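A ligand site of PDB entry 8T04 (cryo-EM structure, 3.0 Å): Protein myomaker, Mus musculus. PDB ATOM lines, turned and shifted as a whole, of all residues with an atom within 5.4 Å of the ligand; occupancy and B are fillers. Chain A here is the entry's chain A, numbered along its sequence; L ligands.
N of Gly 116 lies within hydrogen-bond range of O4 of the ligand, 2.5 Å away. OG of Ser 119 is in hydrogen-bond range of O4 of the ligand (2.6 Å). N of Tyr 118 sits at hydrogen-bond distance from O3 of the ligand (3.0 Å).
N of Gly 161 sits at hydrogen-bond distance from OG of Ser 190 (3.3 Å). The side-chain hydroxyl of Ser 190 is in hydrogen-bond range of the backbone carbonyl oxygen of Gly 157. The backbone carbonyl oxygen (O) of Met 78 lies within hydrogen-bond range of the side-chain hydroxyl (OG) of Ser 81, 3.1 Å away. The backbone carbonyl oxygen of Ser 77 lies within hydrogen-bond range of the side-chain hydroxyl of Ser 81 (2.8 Å). The backbone carbonyl oxygen (O) of Ile 122 sits at hydrogen-bond distance from the side-chain hydroxyl (OG1) of Thr 126, at 2.7 Å. The side-chain hydroxyl (OG1) of Thr 126 is in hydrogen-bond range of the backbone carbonyl oxygen (O) of Gly 123.
The backbone carbonyl oxygen of Trp 113 lies close to a nitrogen (N1) of the ligand. O of Met 78 touches C19 of the ligand, at 3.6 Å. OG of Ser 81 touches C19 of the ligand, at 3.4 Å. Leu 82 touches the ligand. Tyr 115 touches the ligand (C to O4, 3.4 Å). Val 117 touches the ligand. CG2 of Ile 122 touches C7 of the ligand, at 3.6 Å. OG1 of Thr 126 touches C35 of the ligand, at 3.8 Å. Leu 158 touches the ligand. Gly 161 touches the ligand. Ala 162 touches the ligand. Leu 165 touches the ligand (CD1 to C28, 3.9 Å). Phe 169 touches the ligand. Ser 190 touches the ligand (OG to C16, 3.4 Å). CE1 of Phe 191 touches C18 of the ligand, 3.6 Å away. Leu 194 touches the ligand (CD1 to C19, 3.6 Å). Hydrophobic or aromatic side chains within 4 Å of the ligand: Met 78, Leu 82, Tyr 115, Val 117, Tyr 118, Ile 122, Leu 158, Ala 162, Leu 165, Phe 169, Phe 191 and Leu 194. 19 residues have an atom within 4 Å of the ligand: Met 78, Ser 81, Leu 82, Trp 113, Tyr 115, Gly 116, Val 117, Tyr 118, Ser 119, Ile 122, Thr 126, Leu 158, Gly 161, Ala 162, Leu 165, Phe 169, Ser 190, Phe 191 and Leu 194. Along chain A the residues within 4 Å of the ligand span positions 78 to 194. The nearest printed residue that does not touch the ligand is Gly 123 (4.003 Å).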
ATOM      1  N   SER A  77      31.752  -4.666  11.116  1.00  0.00           N
ATOM      2  CA  SER A  77      33.035  -4.677  11.888  1.00  0.00           C
ATOM      3  C   SER A  77      32.805  -5.314  13.258  1.00  0.00           C
ATOM      4  O   SER A  77      33.684  -6.071  13.712  1.00  0.00           O
ATOM      5  CB  SER A  77      33.631  -3.303  12.035  1.00  0.00           C
ATOM      6  OG  SER A  77      33.930  -2.741  10.769  1.00  0.00           O
ATOM      7  N   MET A  78      31.667  -5.002  13.892  1.00  0.00           N
ATOM      8  CA  MET A  78      31.251  -5.557  15.202  1.00  0.00           C
ATOM      9  C   MET A  78      30.994  -7.069  15.073  1.00  0.00           C
ATOM     10  O   MET A  78      31.322  -7.793  16.027  1.00  0.00           O
ATOM     11  CB  MET A  78      29.986  -4.872  15.737  1.00  0.00           C
ATOM     12  CG  MET A  78      30.216  -3.430  16.132  1.00  0.00           C
ATOM     13  SD  MET A  78      28.681  -2.550  16.501  1.00  0.00           S
ATOM     14  CE  MET A  78      29.338  -1.001  17.123  1.00  0.00           C
ATOM     15  N   SER A  81      34.647  -9.040  14.079  1.00  0.00           N
ATOM     16  CA  SER A  81      35.565  -9.010  15.248  1.00  0.00           C
ATOM     17  C   SER A  81      35.125 -10.036  16.294  1.00  0.00           C
ATOM     18  O   SER A  81      36.012 -10.704  16.865  1.00  0.00           O
ATOM     19  CB  SER A  81      35.674  -7.626  15.851  1.00  0.00           C
ATOM     20  OG  SER A  81      34.391  -7.142  16.237  1.00  0.00           O
ATOM     21  N   LEU A  82      33.818 -10.148  16.548  1.00  0.00           N
ATOM     22  CA  LEU A  82      33.245 -11.116  17.526  1.00  0.00           C
ATOM     23  C   LEU A  82      33.304 -12.540  16.948  1.00  0.00           C
ATOM     24  O   LEU A  82      33.560 -13.469  17.739  1.00  0.00           O
ATOM     25  CB  LEU A  82      31.813 -10.715  17.908  1.00  0.00           C
ATOM     26  CG  LEU A  82      31.702  -9.494  18.836  1.00  0.00           C
ATOM     27  CD1 LEU A  82      30.258  -9.046  18.977  1.00  0.00           C
ATOM     28  CD2 LEU A  82      32.296  -9.783  20.207  1.00  0.00           C
ATOM     29  N   TRP A 113      18.530   3.453  11.069  1.00  0.00           N
ATOM     30  CA  TRP A 113      18.446   4.161  12.376  1.00  0.00           C
ATOM     31  C   TRP A 113      17.550   3.424  13.386  1.00  0.00           C
ATOM     32  O   TRP A 113      17.464   3.913  14.516  1.00  0.00           O
ATOM     33  CB  TRP A 113      17.927   5.587  12.186  1.00  0.00           C
ATOM     34  CG  TRP A 113      18.662   6.438  11.209  1.00  0.00           C
ATOM     35  CD1 TRP A 113      18.155   6.963  10.062  1.00  0.00           C
ATOM     36  CD2 TRP A 113      20.021   6.921  11.305  1.00  0.00           C
ATOM     37  NE1 TRP A 113      19.103   7.722   9.423  1.00  0.00           N
ATOM     38  CE2 TRP A 113      20.254   7.712  10.157  1.00  0.00           C
ATOM     39  CE3 TRP A 113      21.064   6.753  12.230  1.00  0.00           C
ATOM     40  CZ2 TRP A 113      21.478   8.327   9.922  1.00  0.00           C
ATOM     41  CZ3 TRP A 113      22.274   7.370  11.996  1.00  0.00           C
ATOM     42  CH2 TRP A 113      22.478   8.151  10.856  1.00  0.00           C
ATOM     43  N   GLY A 114      16.864   2.346  12.991  1.00  0.00           N
ATOM     44  CA  GLY A 114      15.963   1.587  13.881  1.00  0.00           C
ATOM     45  C   GLY A 114      16.736   0.717  14.842  1.00  0.00           C
ATOM     46  O   GLY A 114      17.955   0.532  14.644  1.00  0.00           O
ATOM     47  N   TYR A 115      16.046   0.163  15.855  1.00  0.00           N
ATOM     48  CA  TYR A 115      16.620  -0.700  16.914  1.00  0.00           C
ATOM     49  C   TYR A 115      17.100  -2.013  16.293  1.00  0.00           C
ATOM     50  O   TYR A 115      16.522  -2.448  15.283  1.00  0.00           O
ATOM     51  CB  TYR A 115      15.600  -0.959  18.022  1.00  0.00           C
ATOM     52  CG  TYR A 115      15.042   0.295  18.663  1.00  0.00           C
ATOM     53  CD1 TYR A 115      15.812   1.049  19.531  1.00  0.00           C
ATOM     54  CD2 TYR A 115      13.758   0.736  18.378  1.00  0.00           C
ATOM     55  CE1 TYR A 115      15.321   2.211  20.111  1.00  0.00           C
ATOM     56  CE2 TYR A 115      13.252   1.896  18.950  1.00  0.00           C
ATOM     57  CZ  TYR A 115      14.041   2.628  19.824  1.00  0.00           C
ATOM     58  OH  TYR A 115      13.546   3.770  20.391  1.00  0.00           O
ATOM     59  N   GLY A 116      18.130  -2.636  16.883  1.00  0.00           N
ATOM     60  CA  GLY A 116      18.684  -3.921  16.436  1.00  0.00           C
ATOM     61  C   GLY A 116      19.792  -3.794  15.408  1.00  0.00           C
ATOM     62  O   GLY A 116      20.358  -4.847  15.056  1.00  0.00           O
ATOM     63  N   VAL A 117      20.106  -2.592  14.924  1.00  0.00           N
ATOM     64  CA  VAL A 117      21.123  -2.369  13.841  1.00  0.00           C
ATOM     65  C   VAL A 117      22.537  -2.647  14.393  1.00  0.00           C
ATOM     66  O   VAL A 117      23.378  -3.089  13.588  1.00  0.00           O
ATOM     67  CB  VAL A 117      20.989  -0.993  13.159  1.00  0.00           C
ATOM     68  CG1 VAL A 117      21.251   0.182  14.098  1.00  0.00           C
ATOM     69  CG2 VAL A 117      21.869  -0.883  11.920  1.00  0.00           C
ATOM     70  N   TYR A 118      22.792  -2.415  15.691  1.00  0.00           N
ATOM     71  CA  TYR A 118      24.070  -2.758  16.371  1.00  0.00           C
ATOM     72  C   TYR A 118      23.867  -3.847  17.442  1.00  0.00           C
ATOM     73  O   TYR A 118      24.787  -4.692  17.580  1.00  0.00           O
ATOM     74  CB  TYR A 118      24.724  -1.528  16.993  1.00  0.00           C
ATOM     75  CG  TYR A 118      24.931  -0.379  16.038  1.00  0.00           C
ATOM     76  CD1 TYR A 118      25.912  -0.408  15.063  1.00  0.00           C
ATOM     77  CD2 TYR A 118      24.131   0.750  16.103  1.00  0.00           C
ATOM     78  CE1 TYR A 118      26.102   0.641  14.180  1.00  0.00           C
ATOM     79  CE2 TYR A 118      24.302   1.812  15.228  1.00  0.00           C
ATOM     80  CZ  TYR A 118      25.289   1.765  14.269  1.00  0.00           C
ATOM     81  OH  TYR A 118      25.467   2.810  13.410  1.00  0.00           O
ATOM     82  N   SER A 119      22.747  -3.852  18.169  1.00  0.00           N
ATOM     83  CA  SER A 119      22.430  -4.869  19.218  1.00  0.00           C
ATOM     84  C   SER A 119      22.073  -6.215  18.579  1.00  0.00           C
ATOM     85  O   SER A 119      22.147  -7.234  19.299  1.00  0.00           O
ATOM     86  CB  SER A 119      21.351  -4.402  20.152  1.00  0.00           C
ATOM     87  OG  SER A 119      20.158  -4.112  19.460  1.00  0.00           O
ATOM     88  N   GLY A 120      21.693  -6.230  17.292  1.00  0.00           N
ATOM     89  CA  GLY A 120      21.527  -7.459  16.499  1.00  0.00           C
ATOM     90  C   GLY A 120      22.870  -8.182  16.323  1.00  0.00           C
ATOM     91  O   GLY A 120      23.014  -9.320  16.776  1.00  0.00           O
ATOM     92  N   ILE A 122      25.800  -7.642  17.912  1.00  0.00           N
ATOM     93  CA  ILE A 122      26.480  -7.851  19.221  1.00  0.00           C
ATOM     94  C   ILE A 122      25.699  -8.919  20.016  1.00  0.00           C
ATOM     95  O   ILE A 122      26.344  -9.874  20.498  1.00  0.00           O
ATOM     96  CB  ILE A 122      26.629  -6.532  20.004  1.00  0.00           C
ATOM     97  CG1 ILE A 122      27.525  -5.530  19.251  1.00  0.00           C
ATOM     98  CG2 ILE A 122      27.152  -6.781  21.402  1.00  0.00           C
ATOM     99  CD1 ILE A 122      27.350  -4.093  19.689  1.00  0.00           C
ATOM    100  N   GLY A 123      24.379  -8.756  20.149  1.00  0.00           N
ATOM    101  CA  GLY A 123      23.488  -9.665  20.889  1.00  0.00           C
ATOM    102  C   GLY A 123      23.537 -11.086  20.354  1.00  0.00           C
ATOM    103  O   GLY A 123      23.601 -12.021  21.172  1.00  0.00           O
ATOM    104  N   THR A 126      27.452 -12.585  20.590  1.00  0.00           N
ATOM    105  CA  THR A 126      27.795 -12.939  21.996  1.00  0.00           C
ATOM    106  C   THR A 126      26.995 -14.165  22.455  1.00  0.00           C
ATOM    107  O   THR A 126      27.516 -14.897  23.322  1.00  0.00           O
ATOM    108  CB  THR A 126      27.609 -11.767  22.974  1.00  0.00           C
ATOM    109  OG1 THR A 126      26.289 -11.243  22.813  1.00  0.00           O
ATOM    110  CG2 THR A 126      28.639 -10.672  22.759  1.00  0.00           C
ATOM    111  N   GLY A 157      38.576  -5.834  25.914  1.00  0.00           N
ATOM    112  CA  GLY A 157      37.903  -5.683  24.615  1.00  0.00           C
ATOM    113  C   GLY A 157      36.433  -5.323  24.759  1.00  0.00           C
ATOM    114  O   GLY A 157      35.978  -4.417  24.045  1.00  0.00           O
ATOM    115  N   LEU A 158      35.716  -6.007  25.662  1.00  0.00           N
ATOM    116  CA  LEU A 158      34.269  -5.751  25.938  1.00  0.00           C
ATOM    117  C   LEU A 158      34.107  -4.507  26.811  1.00  0.00           C
ATOM    118  O   LEU A 158      33.021  -3.900  26.740  1.00  0.00           O
ATOM    119  CB  LEU A 158      33.634  -6.984  26.604  1.00  0.00           C
ATOM    120  CG  LEU A 158      33.523  -8.240  25.738  1.00  0.00           C
ATOM    121  CD1 LEU A 158      32.940  -9.393  26.550  1.00  0.00           C
ATOM    122  CD2 LEU A 158      32.673  -8.009  24.497  1.00  0.00           C
ATOM    123  N   GLY A 161      34.482  -1.835  24.276  1.00  0.00           N
ATOM    124  CA  GLY A 161      33.231  -2.007  23.514  1.00  0.00           C
ATOM    125  C   GLY A 161      32.056  -1.328  24.200  1.00  0.00           C
ATOM    126  O   GLY A 161      31.376  -0.527  23.543  1.00  0.00           O
ATOM    127  N   ALA A 162      31.848  -1.623  25.495  1.00  0.00           N
ATOM    128  CA  ALA A 162      30.795  -1.038  26.351  1.00  0.00           C
ATOM    129  C   ALA A 162      30.985   0.480  26.454  1.00  0.00           C
ATOM    130  O   ALA A 162      29.969   1.196  26.430  1.00  0.00           O
ATOM    131  CB  ALA A 162      30.800  -1.681  27.714  1.00  0.00           C
ATOM    132  N   LEU A 165      29.858   2.068  23.086  1.00  0.00           N
ATOM    133  CA  LEU A 165      28.373   2.026  22.950  1.00  0.00           C
ATOM    134  C   LEU A 165      27.721   3.088  23.857  1.00  0.00           C
ATOM    135  O   LEU A 165      26.792   3.757  23.378  1.00  0.00           O
ATOM    136  CB  LEU A 165      27.857   0.612  23.259  1.00  0.00           C
ATOM    137  CG  LEU A 165      28.320  -0.494  22.318  1.00  0.00           C
ATOM    138  CD1 LEU A 165      27.899  -1.856  22.831  1.00  0.00           C
ATOM    139  CD2 LEU A 165      27.803  -0.288  20.892  1.00  0.00           C
ATOM    140  N   MET A 166      28.218   3.291  25.092  1.00  0.00           N
ATOM    141  CA  MET A 166      27.633   4.296  26.033  1.00  0.00           C
ATOM    142  C   MET A 166      28.080   5.715  25.656  1.00  0.00           C
ATOM    143  O   MET A 166      27.313   6.653  25.947  1.00  0.00           O
ATOM    144  CB  MET A 166      27.952   3.991  27.499  1.00  0.00           C
ATOM    145  CG  MET A 166      29.404   4.196  27.911  1.00  0.00           C
ATOM    146  SD  MET A 166      29.678   3.824  29.666  1.00  0.00           S
ATOM    147  CE  MET A 166      29.454   2.048  29.694  1.00  0.00           C
ATOM    148  N   PHE A 169      25.673   6.162  22.305  1.00  0.00           N
ATOM    149  CA  PHE A 169      24.195   5.989  22.507  1.00  0.00           C
ATOM    150  C   PHE A 169      23.695   6.525  23.856  1.00  0.00           C
ATOM    151  O   PHE A 169      22.513   6.266  24.158  1.00  0.00           O
ATOM    152  CB  PHE A 169      23.801   4.520  22.369  1.00  0.00           C
ATOM    153  CG  PHE A 169      24.113   3.923  21.023  1.00  0.00           C
ATOM    154  CD1 PHE A 169      23.492   4.397  19.888  1.00  0.00           C
ATOM    155  CD2 PHE A 169      25.045   2.898  20.893  1.00  0.00           C
ATOM    156  CE1 PHE A 169      23.785   3.863  18.641  1.00  0.00           C
ATOM    157  CE2 PHE A 169      25.339   2.368  19.655  1.00  0.00           C
ATOM    158  CZ  PHE A 169      24.705   2.847  18.530  1.00  0.00           C
ATOM    159  N   PHE A 170      24.511   7.244  24.645  1.00  0.00           N
ATOM    160  CA  PHE A 170      24.055   7.955  25.869  1.00  0.00           C
ATOM    161  C   PHE A 170      24.699   9.341  25.963  1.00  0.00           C
ATOM    162  O   PHE A 170      23.941  10.335  25.985  1.00  0.00           O
ATOM    163  CB  PHE A 170      24.272   7.100  27.122  1.00  0.00           C
ATOM    164  CG  PHE A 170      24.025   7.818  28.425  1.00  0.00           C
ATOM    165  CD1 PHE A 170      22.827   8.489  28.645  1.00  0.00           C
ATOM    166  CD2 PHE A 170      24.980   7.849  29.428  1.00  0.00           C
ATOM    167  CE1 PHE A 170      22.592   9.161  29.834  1.00  0.00           C
ATOM    168  CE2 PHE A 170      24.752   8.514  30.619  1.00  0.00           C
ATOM    169  CZ  PHE A 170      23.552   9.178  30.820  1.00  0.00           C
ATOM    170  N   LEU A 187      35.960   2.313  20.078  1.00  0.00           N
ATOM    171  CA  LEU A 187      35.495   1.179  19.225  1.00  0.00           C
ATOM    172  C   LEU A 187      36.687   0.553  18.484  1.00  0.00           C
ATOM    173  O   LEU A 187      36.724  -0.693  18.402  1.00  0.00           O
ATOM    174  CB  LEU A 187      34.431   1.641  18.226  1.00  0.00           C
ATOM    175  CG  LEU A 187      33.717   0.515  17.478  1.00  0.00           C
ATOM    176  CD1 LEU A 187      32.821  -0.294  18.418  1.00  0.00           C
ATOM    177  CD2 LEU A 187      32.902   1.046  16.315  1.00  0.00           C
ATOM    178  N   SER A 190      38.536  -1.425  20.969  1.00  0.00           N
ATOM    179  CA  SER A 190      37.715  -2.639  21.233  1.00  0.00           C
ATOM    180  C   SER A 190      37.989  -3.698  20.159  1.00  0.00           C
ATOM    181  O   SER A 190      38.193  -4.873  20.533  1.00  0.00           O
ATOM    182  CB  SER A 190      36.250  -2.314  21.325  1.00  0.00           C
ATOM    183  OG  SER A 190      35.488  -3.476  21.604  1.00  0.00           O
ATOM    184  N   PHE A 191      38.005  -3.305  18.885  1.00  0.00           N
ATOM    185  CA  PHE A 191      38.253  -4.197  17.722  1.00  0.00           C
ATOM    186  C   PHE A 191      39.689  -4.757  17.784  1.00  0.00           C
ATOM    187  O   PHE A 191      39.871  -5.914  17.381  1.00  0.00           O
ATOM    188  CB  PHE A 191      38.018  -3.470  16.389  1.00  0.00           C
ATOM    189  CG  PHE A 191      36.596  -3.074  16.063  1.00  0.00           C
ATOM    190  CD1 PHE A 191      35.490  -3.667  16.672  1.00  0.00           C
ATOM    191  CD2 PHE A 191      36.364  -2.119  15.087  1.00  0.00           C
ATOM    192  CE1 PHE A 191      34.201  -3.283  16.333  1.00  0.00           C
ATOM    193  CE2 PHE A 191      35.075  -1.736  14.749  1.00  0.00           C
ATOM    194  CZ  PHE A 191      33.993  -2.318  15.372  1.00  0.00           C
ATOM    195  N   LEU A 194      39.540  -7.416  21.015  1.00  0.00           N
ATOM    196  CA  LEU A 194      38.652  -8.599  20.803  1.00  0.00           C
ATOM    197  C   LEU A 194      39.253  -9.539  19.762  1.00  0.00           C
ATOM    198  O   LEU A 194      39.009 -10.754  19.876  1.00  0.00           O
ATOM    199  CB  LEU A 194      37.253  -8.141  20.387  1.00  0.00           C
ATOM    200  CG  LEU A 194      36.443  -7.427  21.475  1.00  0.00           C
ATOM    201  CD1 LEU A 194      35.206  -6.791  20.875  1.00  0.00           C
ATOM    202  CD2 LEU A 194      36.047  -8.387  22.588  1.00  0.00           C
HETATM  203  C1  LIG L   1      22.131   0.244  20.767  1.00  0.00           C
HETATM  204  N1  LIG L   1      18.882   4.275  17.655  1.00  0.00           N
HETATM  205  P1  LIG L   1      20.555  -0.542  18.781  1.00  0.00           P
HETATM  206  C2  LIG L   1      22.246  -0.105  22.255  1.00  0.00           C
HETATM  207  C3  LIG L   1      21.916   1.138  23.096  1.00  0.00           C
HETATM  208  C4  LIG L   1      29.769  -5.524  24.947  1.00  0.00           C
HETATM  209  C5  LIG L   1      27.523  -9.018  27.244  1.00  0.00           C
HETATM  210  C6  LIG L   1      18.671   2.867  18.093  1.00  0.00           C
HETATM  211  O1  LIG L   1      21.503  -0.838  20.120  1.00  0.00           O
HETATM  212  C7  LIG L   1      29.994  -5.840  23.435  1.00  0.00           C
HETATM  213  C8  LIG L   1      28.856  -9.814  27.332  1.00  0.00           C
HETATM  214  C9  LIG L   1      19.943   1.966  18.067  1.00  0.00           C
HETATM  215  O2  LIG L   1      19.730   0.900  18.959  1.00  0.00           O
HETATM  216  C10 LIG L   1      30.836  -4.723  22.785  1.00  0.00           C
HETATM  217  C11 LIG L   1      28.748 -10.865  28.452  1.00  0.00           C
HETATM  218  C12 LIG L   1      17.569   4.860  17.460  1.00  0.00           C
HETATM  219  O3  LIG L   1      21.420  -0.537  17.540  1.00  0.00           O
HETATM  220  C13 LIG L   1      31.099  -5.090  21.308  1.00  0.00           C
HETATM  221  C14 LIG L   1      27.523 -11.789  28.221  1.00  0.00           C
HETATM  222  C15 LIG L   1      19.681   4.340  16.454  1.00  0.00           C
HETATM  223  O4  LIG L   1      19.549  -1.657  18.689  1.00  0.00           O
HETATM  224  C16 LIG L   1      32.311  -4.274  20.818  1.00  0.00           C
HETATM  225  C17 LIG L   1      19.534   5.057  18.700  1.00  0.00           C
HETATM  226  C18 LIG L   1      32.464  -4.337  19.287  1.00  0.00           C
HETATM  227  C19 LIG L   1      32.537  -5.769  18.731  1.00  0.00           C
HETATM  228  C20 LIG L   1      22.637   1.841  25.288  1.00  0.00           C
HETATM  229  O5  LIG L   1      22.050   0.830  24.480  1.00  0.00           O
HETATM  230  C21 LIG L   1      23.905   1.525  26.152  1.00  0.00           C
HETATM  231  O6  LIG L   1      22.179   2.924  25.314  1.00  0.00           O
HETATM  232  C22 LIG L   1      24.324   0.043  25.988  1.00  0.00           C
HETATM  233  C23 LIG L   1      25.540  -0.261  26.908  1.00  0.00           C
HETATM  234  C24 LIG L   1      26.340  -1.486  26.375  1.00  0.00           C
HETATM  235  C25 LIG L   1      26.483  -2.583  27.490  1.00  0.00           C
HETATM  236  C26 LIG L   1      26.757  -3.978  26.852  1.00  0.00           C
HETATM  237  C27 LIG L   1      28.246  -4.106  26.426  1.00  0.00           C
HETATM  238  C28 LIG L   1      28.334  -4.933  25.109  1.00  0.00           C
HETATM  239  C29 LIG L   1      23.854  -1.882  22.271  1.00  0.00           C
HETATM  240  O7  LIG L   1      23.562  -0.511  22.523  1.00  0.00           O
HETATM  241  C30 LIG L   1      24.069  -2.829  23.482  1.00  0.00           C
HETATM  242  O8  LIG L   1      23.962  -2.283  21.159  1.00  0.00           O
HETATM  243  C31 LIG L   1      23.197  -4.112  23.391  1.00  0.00           C
HETATM  244  C32 LIG L   1      24.068  -5.355  23.725  1.00  0.00           C
HETATM  245  C33 LIG L   1      23.249  -6.652  23.514  1.00  0.00           C
HETATM  246  C34 LIG L   1      23.592  -7.697  24.606  1.00  0.00           C
HETATM  247  C35 LIG L   1      25.099  -8.070  24.601  1.00  0.00           C
HETATM  248  C36 LIG L   1      25.727  -7.838  25.991  1.00  0.00           C
HETATM  249  C37 LIG L   1      27.053  -8.617  26.062  1.00  0.00           C
